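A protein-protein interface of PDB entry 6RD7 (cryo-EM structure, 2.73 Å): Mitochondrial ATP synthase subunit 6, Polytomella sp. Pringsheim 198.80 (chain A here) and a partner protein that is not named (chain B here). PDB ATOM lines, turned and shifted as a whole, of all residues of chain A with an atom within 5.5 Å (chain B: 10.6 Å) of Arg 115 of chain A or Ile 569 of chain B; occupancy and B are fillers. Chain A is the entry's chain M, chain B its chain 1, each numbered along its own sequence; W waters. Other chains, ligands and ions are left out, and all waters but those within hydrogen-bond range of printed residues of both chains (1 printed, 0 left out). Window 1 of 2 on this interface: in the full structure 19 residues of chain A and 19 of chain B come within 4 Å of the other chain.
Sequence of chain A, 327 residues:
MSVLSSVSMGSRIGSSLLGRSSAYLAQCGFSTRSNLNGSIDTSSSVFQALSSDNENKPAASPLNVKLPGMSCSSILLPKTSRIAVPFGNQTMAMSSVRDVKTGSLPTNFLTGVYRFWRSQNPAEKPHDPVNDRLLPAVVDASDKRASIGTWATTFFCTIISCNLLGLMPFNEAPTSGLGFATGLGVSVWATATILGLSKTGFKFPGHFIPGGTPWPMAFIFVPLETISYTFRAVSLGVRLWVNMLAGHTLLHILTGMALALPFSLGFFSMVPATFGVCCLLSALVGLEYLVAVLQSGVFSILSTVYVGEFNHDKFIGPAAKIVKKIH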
ATOM      1  N   LEU A 110     -25.135  -7.045   0.690  1.00  0.00           N
ATOM      2  CA  LEU A 110     -26.464  -6.873   0.129  1.00  0.00           C
ATOM      3  C   LEU A 110     -26.421  -6.066  -1.159  1.00  0.00           C
ATOM      4  O   LEU A 110     -27.253  -6.273  -2.047  1.00  0.00           O
ATOM      5  CB  LEU A 110     -27.353  -6.206   1.162  1.00  0.00           C
ATOM      6  CG  LEU A 110     -28.841  -6.496   1.121  1.00  0.00           C
ATOM      7  CD1 LEU A 110     -29.098  -7.984   1.097  1.00  0.00           C
ATOM      8  CD2 LEU A 110     -29.416  -5.887   2.359  1.00  0.00           C
ATOM      9  N   THR A 111     -25.444  -5.165  -1.286  1.00  0.00           N
ATOM     10  CA  THR A 111     -25.219  -4.467  -2.546  1.00  0.00           C
ATOM     11  C   THR A 111     -24.811  -5.439  -3.638  1.00  0.00           C
ATOM     12  O   THR A 111     -25.352  -5.395  -4.748  1.00  0.00           O
ATOM     13  CB  THR A 111     -24.140  -3.404  -2.369  1.00  0.00           C
ATOM     14  OG1 THR A 111     -24.426  -2.620  -1.210  1.00  0.00           O
ATOM     15  CG2 THR A 111     -24.083  -2.504  -3.580  1.00  0.00           C
ATOM     16  N   GLY A 112     -23.873  -6.338  -3.329  1.00  0.00           N
ATOM     17  CA  GLY A 112     -23.463  -7.335  -4.307  1.00  0.00           C
ATOM     18  C   GLY A 112     -24.571  -8.303  -4.673  1.00  0.00           C
ATOM     19  O   GLY A 112     -24.722  -8.669  -5.840  1.00  0.00           O
ATOM     20  N   VAL A 113     -25.396  -8.685  -3.693  1.00  0.00           N
ATOM     21  CA  VAL A 113     -26.503  -9.606  -3.945  1.00  0.00           C
ATOM     22  C   VAL A 113     -27.568  -8.946  -4.818  1.00  0.00           C
ATOM     23  O   VAL A 113     -28.044  -9.540  -5.796  1.00  0.00           O
ATOM     24  CB  VAL A 113     -27.080 -10.113  -2.610  1.00  0.00           C
ATOM     25  CG1 VAL A 113     -28.486 -10.645  -2.772  1.00  0.00           C
ATOM     26  CG2 VAL A 113     -26.196 -11.191  -2.037  1.00  0.00           C
ATOM     27  N   TYR A 114     -27.931  -7.696  -4.500  1.00  0.00           N
ATOM     28  CA  TYR A 114     -28.929  -6.986  -5.293  1.00  0.00           C
ATOM     29  C   TYR A 114     -28.431  -6.714  -6.704  1.00  0.00           C
ATOM     30  O   TYR A 114     -29.201  -6.799  -7.663  1.00  0.00           O
ATOM     31  CB  TYR A 114     -29.320  -5.671  -4.621  1.00  0.00           C
ATOM     32  CG  TYR A 114     -30.248  -4.842  -5.481  1.00  0.00           C
ATOM     33  CD1 TYR A 114     -31.575  -5.208  -5.636  1.00  0.00           C
ATOM     34  CD2 TYR A 114     -29.795  -3.714  -6.156  1.00  0.00           C
ATOM     35  CE1 TYR A 114     -32.424  -4.477  -6.426  1.00  0.00           C
ATOM     36  CE2 TYR A 114     -30.642  -2.980  -6.956  1.00  0.00           C
ATOM     37  CZ  TYR A 114     -31.956  -3.368  -7.084  1.00  0.00           C
ATOM     38  OH  TYR A 114     -32.816  -2.643  -7.871  1.00  0.00           O
ATOM     39  N   ARG A 115     -27.147  -6.387  -6.853  1.00  0.00           N
ATOM     40  CA  ARG A 115     -26.622  -6.124  -8.185  1.00  0.00           C
ATOM     41  C   ARG A 115     -26.455  -7.412  -8.974  1.00  0.00           C
ATOM     42  O   ARG A 115     -26.434  -7.390 -10.207  1.00  0.00           O
ATOM     43  CB  ARG A 115     -25.303  -5.373  -8.084  1.00  0.00           C
ATOM     44  CG  ARG A 115     -25.472  -3.932  -7.702  1.00  0.00           C
ATOM     45  CD  ARG A 115     -24.137  -3.300  -7.427  1.00  0.00           C
ATOM     46  NE  ARG A 115     -23.274  -3.358  -8.596  1.00  0.00           N
ATOM     47  CZ  ARG A 115     -23.275  -2.457  -9.570  1.00  0.00           C
ATOM     48  NH1 ARG A 115     -22.453  -2.596 -10.596  1.00  0.00           N
ATOM     49  NH2 ARG A 115     -24.094  -1.420  -9.518  1.00  0.00           N
ATOM     50  N   PHE A 116     -26.337  -8.547  -8.282  1.00  0.00           N
ATOM     51  CA  PHE A 116     -26.352  -9.829  -8.972  1.00  0.00           C
ATOM     52  C   PHE A 116     -27.744 -10.157  -9.494  1.00  0.00           C
ATOM     53  O   PHE A 116     -27.899 -10.598 -10.635  1.00  0.00           O
ATOM     54  CB  PHE A 116     -25.857 -10.933  -8.042  1.00  0.00           C
ATOM     55  CG  PHE A 116     -25.828 -12.288  -8.678  1.00  0.00           C
ATOM     56  CD1 PHE A 116     -24.838 -12.618  -9.583  1.00  0.00           C
ATOM     57  CD2 PHE A 116     -26.793 -13.230  -8.375  1.00  0.00           C
ATOM     58  CE1 PHE A 116     -24.811 -13.862 -10.171  1.00  0.00           C
ATOM     59  CE2 PHE A 116     -26.772 -14.473  -8.960  1.00  0.00           C
ATOM     60  CZ  PHE A 116     -25.779 -14.789  -9.858  1.00  0.00           C
ATOM     61  N   TRP A 117     -28.775  -9.955  -8.668  1.00  0.00           N
ATOM     62  CA  TRP A 117     -30.124 -10.322  -9.104  1.00  0.00           C
ATOM     63  C   TRP A 117     -30.687  -9.318 -10.096  1.00  0.00           C
ATOM     64  O   TRP A 117     -31.551  -9.658 -10.909  1.00  0.00           O
ATOM     65  CB  TRP A 117     -31.060 -10.480  -7.906  1.00  0.00           C
ATOM     66  CG  TRP A 117     -30.673 -11.620  -7.012  1.00  0.00           C
ATOM     67  CD1 TRP A 117     -30.346 -11.536  -5.705  1.00  0.00           C
ATOM     68  CD2 TRP A 117     -30.542 -13.006  -7.370  1.00  0.00           C
ATOM     69  NE1 TRP A 117     -30.027 -12.775  -5.214  1.00  0.00           N
ATOM     70  CE2 TRP A 117     -30.140 -13.696  -6.218  1.00  0.00           C
ATOM     71  CE3 TRP A 117     -30.734 -13.729  -8.552  1.00  0.00           C
ATOM     72  CZ2 TRP A 117     -29.925 -15.066  -6.212  1.00  0.00           C
ATOM     73  CZ3 TRP A 117     -30.531 -15.064  -8.535  1.00  0.00           C
ATOM     74  CH2 TRP A 117     -30.109 -15.729  -7.387  1.00  0.00           C
ATOM     75  N   ARG A 118     -30.217  -8.076 -10.038  1.00  0.00           N
ATOM     76  CA  ARG A 118     -30.586  -7.075 -11.026  1.00  0.00           C
ATOM     77  C   ARG A 118     -29.931  -7.352 -12.372  1.00  0.00           C
ATOM     78  O   ARG A 118     -30.520  -7.046 -13.412  1.00  0.00           O
ATOM     79  CB  ARG A 118     -30.217  -5.694 -10.475  1.00  0.00           C
ATOM     80  CG  ARG A 118     -30.387  -4.501 -11.394  1.00  0.00           C
ATOM     81  CD  ARG A 118     -31.772  -4.398 -12.002  1.00  0.00           C
ATOM     82  NE  ARG A 118     -31.797  -3.418 -13.084  1.00  0.00           N
ATOM     83  CZ  ARG A 118     -31.368  -3.641 -14.321  1.00  0.00           C
ATOM     84  NH1 ARG A 118     -30.879  -4.823 -14.665  1.00  0.00           N
ATOM     85  NH2 ARG A 118     -31.433  -2.678 -15.224  1.00  0.00           N
ATOM     86  N   SER A 119     -28.757  -7.974 -12.383  1.00  0.00           N
ATOM     87  CA  SER A 119     -28.063  -8.278 -13.625  1.00  0.00           C
ATOM     88  C   SER A 119     -28.614  -9.500 -14.345  1.00  0.00           C
ATOM     89  O   SER A 119     -28.118  -9.835 -15.423  1.00  0.00           O
ATOM     90  CB  SER A 119     -26.573  -8.488 -13.358  1.00  0.00           C
ATOM     91  OG  SER A 119     -26.329  -9.796 -12.881  1.00  0.00           O
ATOM     92  N   GLU B 559     -34.393   9.128  -6.591  1.00  0.00           N
ATOM     93  CA  GLU B 559     -34.200   7.958  -7.443  1.00  0.00           C
ATOM     94  C   GLU B 559     -34.758   6.699  -6.799  1.00  0.00           C
ATOM     95  O   GLU B 559     -35.384   5.876  -7.473  1.00  0.00           O
ATOM     96  CB  GLU B 559     -32.722   7.769  -7.750  1.00  0.00           C
ATOM     97  CG  GLU B 559     -32.293   8.320  -9.070  1.00  0.00           C
ATOM     98  CD  GLU B 559     -30.818   8.135  -9.315  1.00  0.00           C
ATOM     99  OE1 GLU B 559     -30.446   7.176 -10.017  1.00  0.00           O
ATOM    100  OE2 GLU B 559     -30.024   8.941  -8.796  1.00  0.00           O
ATOM    101  N   ALA B 563     -38.624   4.473  -8.065  1.00  0.00           N
ATOM    102  CA  ALA B 563     -38.350   3.130  -8.592  1.00  0.00           C
ATOM    103  C   ALA B 563     -37.251   3.140  -9.649  1.00  0.00           C
ATOM    104  O   ALA B 563     -37.253   2.346 -10.589  1.00  0.00           O
ATOM    105  CB  ALA B 563     -39.621   2.469  -9.127  1.00  0.00           C
ATOM    106  N   LEU B 564     -36.301   4.052  -9.490  1.00  0.00           N
ATOM    107  CA  LEU B 564     -35.148   4.159 -10.370  1.00  0.00           C
ATOM    108  C   LEU B 564     -33.862   3.901  -9.605  1.00  0.00           C
ATOM    109  O   LEU B 564     -32.843   4.537  -9.865  1.00  0.00           O
ATOM    110  CB  LEU B 564     -35.097   5.529 -11.039  1.00  0.00           C
ATOM    111  CG  LEU B 564     -36.183   5.837 -12.059  1.00  0.00           C
ATOM    112  CD1 LEU B 564     -36.284   7.330 -12.255  1.00  0.00           C
ATOM    113  CD2 LEU B 564     -35.883   5.144 -13.366  1.00  0.00           C
ATOM    114  N   GLU B 565     -33.902   2.979  -8.643  1.00  0.00           N
ATOM    115  CA  GLU B 565     -32.717   2.691  -7.851  1.00  0.00           C
ATOM    116  C   GLU B 565     -31.650   1.966  -8.659  1.00  0.00           C
ATOM    117  O   GLU B 565     -30.467   2.063  -8.331  1.00  0.00           O
ATOM    118  CB  GLU B 565     -33.097   1.887  -6.608  1.00  0.00           C
ATOM    119  CG  GLU B 565     -33.607   0.494  -6.887  1.00  0.00           C
ATOM    120  CD  GLU B 565     -35.114   0.437  -6.954  1.00  0.00           C
ATOM    121  OE1 GLU B 565     -35.753   1.503  -6.882  1.00  0.00           O
ATOM    122  OE2 GLU B 565     -35.662  -0.674  -7.082  1.00  0.00           O
ATOM    123  N   ASP B 566     -32.032   1.291  -9.736  1.00  0.00           N
ATOM    124  CA  ASP B 566     -31.088   0.621 -10.612  1.00  0.00           C
ATOM    125  C   ASP B 566     -30.818   1.422 -11.875  1.00  0.00           C
ATOM    126  O   ASP B 566     -30.565   0.833 -12.928  1.00  0.00           O
ATOM    127  CB  ASP B 566     -31.608  -0.767 -10.973  1.00  0.00           C
ATOM    128  CG  ASP B 566     -32.994  -0.725 -11.596  1.00  0.00           C
ATOM    129  OD1 ASP B 566     -33.831   0.080 -11.144  1.00  0.00           O
ATOM    130  OD2 ASP B 566     -33.250  -1.497 -12.541  1.00  0.00           O
ATOM    131  N   PHE B 567     -30.868   2.755 -11.795  1.00  0.00           N
ATOM    132  CA  PHE B 567     -30.805   3.559 -13.010  1.00  0.00           C
ATOM    133  C   PHE B 567     -29.398   3.605 -13.582  1.00  0.00           C
ATOM    134  O   PHE B 567     -29.223   3.611 -14.804  1.00  0.00           O
ATOM    135  CB  PHE B 567     -31.314   4.973 -12.755  1.00  0.00           C
ATOM    136  CG  PHE B 567     -31.414   5.795 -13.998  1.00  0.00           C
ATOM    137  CD1 PHE B 567     -32.289   5.433 -15.005  1.00  0.00           C
ATOM    138  CD2 PHE B 567     -30.616   6.910 -14.176  1.00  0.00           C
ATOM    139  CE1 PHE B 567     -32.380   6.174 -16.160  1.00  0.00           C
ATOM    140  CE2 PHE B 567     -30.704   7.655 -15.332  1.00  0.00           C
ATOM    141  CZ  PHE B 567     -31.585   7.283 -16.325  1.00  0.00           C
ATOM    142  N   ASP B 568     -28.379   3.635 -12.723  1.00  0.00           N
ATOM    143  CA  ASP B 568     -27.015   3.555 -13.231  1.00  0.00           C
ATOM    144  C   ASP B 568     -26.703   2.156 -13.746  1.00  0.00           C
ATOM    145  O   ASP B 568     -25.927   2.003 -14.693  1.00  0.00           O
ATOM    146  CB  ASP B 568     -26.019   3.987 -12.157  1.00  0.00           C
ATOM    147  CG  ASP B 568     -25.929   3.009 -11.010  1.00  0.00           C
ATOM    148  OD1 ASP B 568     -26.952   2.788 -10.334  1.00  0.00           O
ATOM    149  OD2 ASP B 568     -24.831   2.467 -10.780  1.00  0.00           O
ATOM    150  N   ILE B 569     -27.344   1.134 -13.177  1.00  0.00           N
ATOM    151  CA  ILE B 569     -27.244  -0.214 -13.727  1.00  0.00           C
ATOM    152  C   ILE B 569     -27.945  -0.287 -15.078  1.00  0.00           C
ATOM    153  O   ILE B 569     -27.478  -0.964 -15.998  1.00  0.00           O
ATOM    154  CB  ILE B 569     -27.817  -1.234 -12.726  1.00  0.00           C
ATOM    155  CG1 ILE B 569     -27.159  -1.065 -11.360  1.00  0.00           C
ATOM    156  CG2 ILE B 569     -27.612  -2.653 -13.214  1.00  0.00           C
ATOM    157  CD1 ILE B 569     -27.706  -1.989 -10.306  1.00  0.00           C
ATOM    158  N   THR B 570     -29.062   0.432 -15.222  1.00  0.00           N
ATOM    159  CA  THR B 570     -29.773   0.485 -16.495  1.00  0.00           C
ATOM    160  C   THR B 570     -28.945   1.194 -17.562  1.00  0.00           C
ATOM    161  O   THR B 570     -28.888   0.747 -18.713  1.00  0.00           O
ATOM    162  CB  THR B 570     -31.123   1.177 -16.293  1.00  0.00           C
ATOM    163  OG1 THR B 570     -31.925   0.396 -15.404  1.00  0.00           O
ATOM    164  CG2 THR B 570     -31.872   1.342 -17.598  1.00  0.00           C
ATOM    165  N   LEU B 571     -28.263   2.276 -17.189  1.00  0.00           N
ATOM    166  CA  LEU B 571     -27.382   2.956 -18.132  1.00  0.00           C
ATOM    167  C   LEU B 571     -26.138   2.134 -18.441  1.00  0.00           C
ATOM    168  O   LEU B 571     -25.556   2.280 -19.518  1.00  0.00           O
ATOM    169  CB  LEU B 571     -26.984   4.326 -17.589  1.00  0.00           C
ATOM    170  CG  LEU B 571     -28.100   5.348 -17.393  1.00  0.00           C
ATOM    171  CD1 LEU B 571     -27.554   6.576 -16.706  1.00  0.00           C
ATOM    172  CD2 LEU B 571     -28.749   5.708 -18.709  1.00  0.00           C
ATOM    173  N   ASP B 572     -25.711   1.277 -17.513  1.00  0.00           N
ATOM    174  CA  ASP B 572     -24.642   0.332 -17.814  1.00  0.00           C
ATOM    175  C   ASP B 572     -25.111  -0.762 -18.764  1.00  0.00           C
ATOM    176  O   ASP B 572     -24.318  -1.272 -19.561  1.00  0.00           O
ATOM    177  CB  ASP B 572     -24.116  -0.294 -16.525  1.00  0.00           C
ATOM    178  CG  ASP B 572     -23.123   0.589 -15.815  1.00  0.00           C
ATOM    179  OD1 ASP B 572     -22.655   1.570 -16.426  1.00  0.00           O
ATOM    180  OD2 ASP B 572     -22.807   0.303 -14.641  1.00  0.00           O
ATOM    181  N   ASP B 573     -26.386  -1.144 -18.675  1.00  0.00           N
ATOM    182  CA  ASP B 573     -26.914  -2.204 -19.528  1.00  0.00           C
ATOM    183  C   ASP B 573     -27.029  -1.745 -20.973  1.00  0.00           C
ATOM    184  O   ASP B 573     -26.772  -2.517 -21.903  1.00  0.00           O
ATOM    185  CB  ASP B 573     -28.278  -2.663 -19.016  1.00  0.00           C
ATOM    186  CG  ASP B 573     -28.183  -3.466 -17.744  1.00  0.00           C
ATOM    187  OD1 ASP B 573     -27.097  -4.009 -17.462  1.00  0.00           O
ATOM    188  OD2 ASP B 573     -29.196  -3.556 -17.022  1.00  0.00           O
ATOM    189  N   MET B 574     -27.411  -0.493 -21.182  1.00  0.00           N
ATOM    190  CA  MET B 574     -27.551   0.065 -22.515  1.00  0.00           C
ATOM    191  C   MET B 574     -26.234   0.551 -23.095  1.00  0.00           C
ATOM    192  O   MET B 574     -26.213   1.018 -24.238  1.00  0.00           O
ATOM    193  CB  MET B 574     -28.560   1.213 -22.490  1.00  0.00           C
ATOM    194  CG  MET B 574     -29.895   0.821 -21.906  1.00  0.00           C
ATOM    195  SD  MET B 574     -30.998   2.215 -21.661  1.00  0.00           S
ATOM    196  CE  MET B 574     -32.560   1.361 -21.523  1.00  0.00           C
ATOM    197  N   GLY B 575     -25.142   0.456 -22.342  1.00  0.00           N
ATOM    198  CA  GLY B 575     -23.851   0.934 -22.811  1.00  0.00           C
ATOM    199  C   GLY B 575     -23.775   2.439 -22.938  1.00  0.00           C
ATOM    200  O   GLY B 575     -22.918   2.958 -23.662  1.00  0.00           O
ATOM    201  N   ALA B 576     -24.657   3.155 -22.244  1.00  0.00           N
ATOM    202  CA  ALA B 576     -24.772   4.603 -22.383  1.00  0.00           C
ATOM    203  C   ALA B 576     -23.758   5.259 -21.455  1.00  0.00           C
ATOM    204  O   ALA B 576     -24.030   5.566 -20.295  1.00  0.00           O
ATOM    205  CB  ALA B 576     -26.193   5.053 -22.084  1.00  0.00           C
ATOM    206  N   GLU B 577     -22.557   5.473 -21.990  1.00  0.00           N
ATOM    207  CA  GLU B 577     -21.494   6.068 -21.189  1.00  0.00           C
ATOM    208  C   GLU B 577     -21.695   7.567 -21.036  1.00  0.00           C
ATOM    209  O   GLU B 577     -21.431   8.129 -19.967  1.00  0.00           O
ATOM    210  CB  GLU B 577     -20.136   5.768 -21.819  1.00  0.00           C
ATOM    211  CG  GLU B 577     -19.950   4.317 -22.212  1.00  0.00           C
ATOM    212  CD  GLU B 577     -19.293   3.493 -21.124  1.00  0.00           C
ATOM    213  OE1 GLU B 577     -18.782   2.398 -21.437  1.00  0.00           O
ATOM    214  OE2 GLU B 577     -19.283   3.935 -19.957  1.00  0.00           O
ATOM    215  N   ALA B 579     -24.614   9.109 -21.143  1.00  0.00           N
ATOM    216  CA  ALA B 579     -25.765   9.316 -20.272  1.00  0.00           C
ATOM    217  C   ALA B 579     -25.412   9.043 -18.817  1.00  0.00           C
ATOM    218  O   ALA B 579     -25.942   9.697 -17.918  1.00  0.00           O
ATOM    219  CB  ALA B 579     -26.931   8.442 -20.717  1.00  0.00           C
ATOM    220  N   LYS B 580     -24.497   8.106 -18.564  1.00  0.00           N
ATOM    221  CA  LYS B 580     -24.063   7.853 -17.194  1.00  0.00           C
ATOM    222  C   LYS B 580     -23.179   8.983 -16.684  1.00  0.00           C
ATOM    223  O   LYS B 580     -23.267   9.378 -15.512  1.00  0.00           O
ATOM    224  CB  LYS B 580     -23.328   6.518 -17.123  1.00  0.00           C
ATOM    225  CG  LYS B 580     -22.957   6.081 -15.726  1.00  0.00           C
ATOM    226  CD  LYS B 580     -22.186   4.783 -15.772  1.00  0.00           C
ATOM    227  CE  LYS B 580     -21.601   4.429 -14.421  1.00  0.00           C
ATOM    228  NZ  LYS B 580     -22.650   4.122 -13.416  1.00  0.00           N
ATOM    229  N   TRP B 583     -25.566  11.679 -15.903  1.00  0.00           N
ATOM    230  CA  TRP B 583     -26.295  11.372 -14.676  1.00  0.00           C
ATOM    231  C   TRP B 583     -25.469  11.714 -13.446  1.00  0.00           C
ATOM    232  O   TRP B 583     -25.970  12.348 -12.503  1.00  0.00           O
ATOM    233  CB  TRP B 583     -26.674   9.893 -14.683  1.00  0.00           C
ATOM    234  CG  TRP B 583     -27.035   9.293 -13.366  1.00  0.00           C
ATOM    235  CD1 TRP B 583     -28.252   9.322 -12.763  1.00  0.00           C
ATOM    236  CD2 TRP B 583     -26.182   8.530 -12.510  1.00  0.00           C
ATOM    237  NE1 TRP B 583     -28.207   8.643 -11.575  1.00  0.00           N
ATOM    238  CE2 TRP B 583     -26.945   8.147 -11.396  1.00  0.00           C
ATOM    239  CE3 TRP B 583     -24.840   8.147 -12.572  1.00  0.00           C
ATOM    240  CZ2 TRP B 583     -26.417   7.396 -10.355  1.00  0.00           C
ATOM    241  CZ3 TRP B 583     -24.318   7.405 -11.539  1.00  0.00           C
ATOM    242  CH2 TRP B 583     -25.103   7.034 -10.446  1.00  0.00           C
ATOM    243  N   ASN B 587     -26.281  14.867 -10.858  1.00  0.00           N
ATOM    244  CA  ASN B 587     -26.538  14.633  -9.443  1.00  0.00           C
ATOM    245  C   ASN B 587     -25.615  15.464  -8.564  1.00  0.00           C
ATOM    246  O   ASN B 587     -25.904  15.684  -7.385  1.00  0.00           O
ATOM    247  CB  ASN B 587     -26.401  13.158  -9.112  1.00  0.00           C
ATOM    248  CG  ASN B 587     -27.614  12.360  -9.511  1.00  0.00           C
ATOM    249  OD1 ASN B 587     -28.734  12.858  -9.488  1.00  0.00           O
ATOM    250  ND2 ASN B 587     -27.401  11.107  -9.867  1.00  0.00           N
HETATM  251  O   HOH W   1     -23.480   0.457 -11.923  1.00  0.00           O
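The guanidinium group of Arg 118 of chain A is in salt-bridge range of the side-chain carboxylate of Asp 566 of chain B, at 2.5 Å. OG1 of Thr 570 of chain B lies within hydrogen-bond range of NH2 of Arg 118 of chain A. OD2 of Asp 573 of chain B is in salt-bridge range of NH2 of Arg 118 of chain A.
The backbone NH (N) of Glu 565 of chain B lies within hydrogen-bond range of the backbone carbonyl oxygen (O) of Glu 559 of chain B (3.5 Å). O of Asp 566 of chain B lies within hydrogen-bond range of OG1 of Thr 570 of chain B, at 2.9 Å.
Among the printed residues, merely in contact across the chains: Tyr 114 of chain A with Glu 565 of chain B, Tyr 114 of chain A with Asp 566 of chain B, Arg 115 of chain A with Ile 569 of chain B and Arg 118 of chain A with Ile 569 of chain B.
Leu 110 of chain A touches none of the printed residues of chain B. No residue of chain B comes within 4 Å of Gly 112 of chain A. Arg 115 of chain A touches just one residue of chain B: Ile 569 (3.6 Å). Phe 116 of chain A touches none of the printed residues of chain B. Arg 118 of chain A touches just these residues of chain B: Asp 566, Ile 569, Thr 570 and Asp 573. No residue of chain B comes within 4 Å of Ser 119 of chain A. Printed residues of chain A within 4 Å of Glu 565 of chain B: Tyr 114 (3.4 Å). Of the printed residues of chain A, Asp 566 of chain B touches Tyr 114 (3.8 Å) and Arg 118 (2.5 Å). Ile 569 of chain B touches just these residues of chain A: Arg 115 and Arg 118. Of the printed residues of chain A, Thr 570 of chain B touches Arg 118 (3.1 Å). Printed residues of chain A within 4 Å of Asp 573 of chain B: Arg 118. The nearest residue of chain A that does not touch Ile 569 of chain B is Tyr 114 of chain A (4.6 Å).
Hydrophobic or aromatic side chains of chain B within 4 Å of the printed part of chain A: Ile 569. Of the 10 printed residues of chain A, 3 touch a printed residue of chain B. Printed residues of chain A that touch a printed residue of chain B: Tyr 114, Arg 115 and Arg 118. Hydrophobic or aromatic side chains of chain A within 4 Å of the printed part of chain B: Tyr 114. Among the printed residues, Asp or Glu carboxylates within 4 Å of a Lys or Arg side-chain nitrogen of the other chain: Arg 118 of chain A with Asp 566 of chain B (2.5 Å) and Arg 118 of chain A with Asp 573 of chain B (3.0 Å).
Water W1 lies within hydrogen-bond range of OD2 of Asp 568 of chain B (2.7 Å), OD2 of Asp 572 of chain B (2.8 Å) and NH2 of Arg 115 of chain A (3.1 Å).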
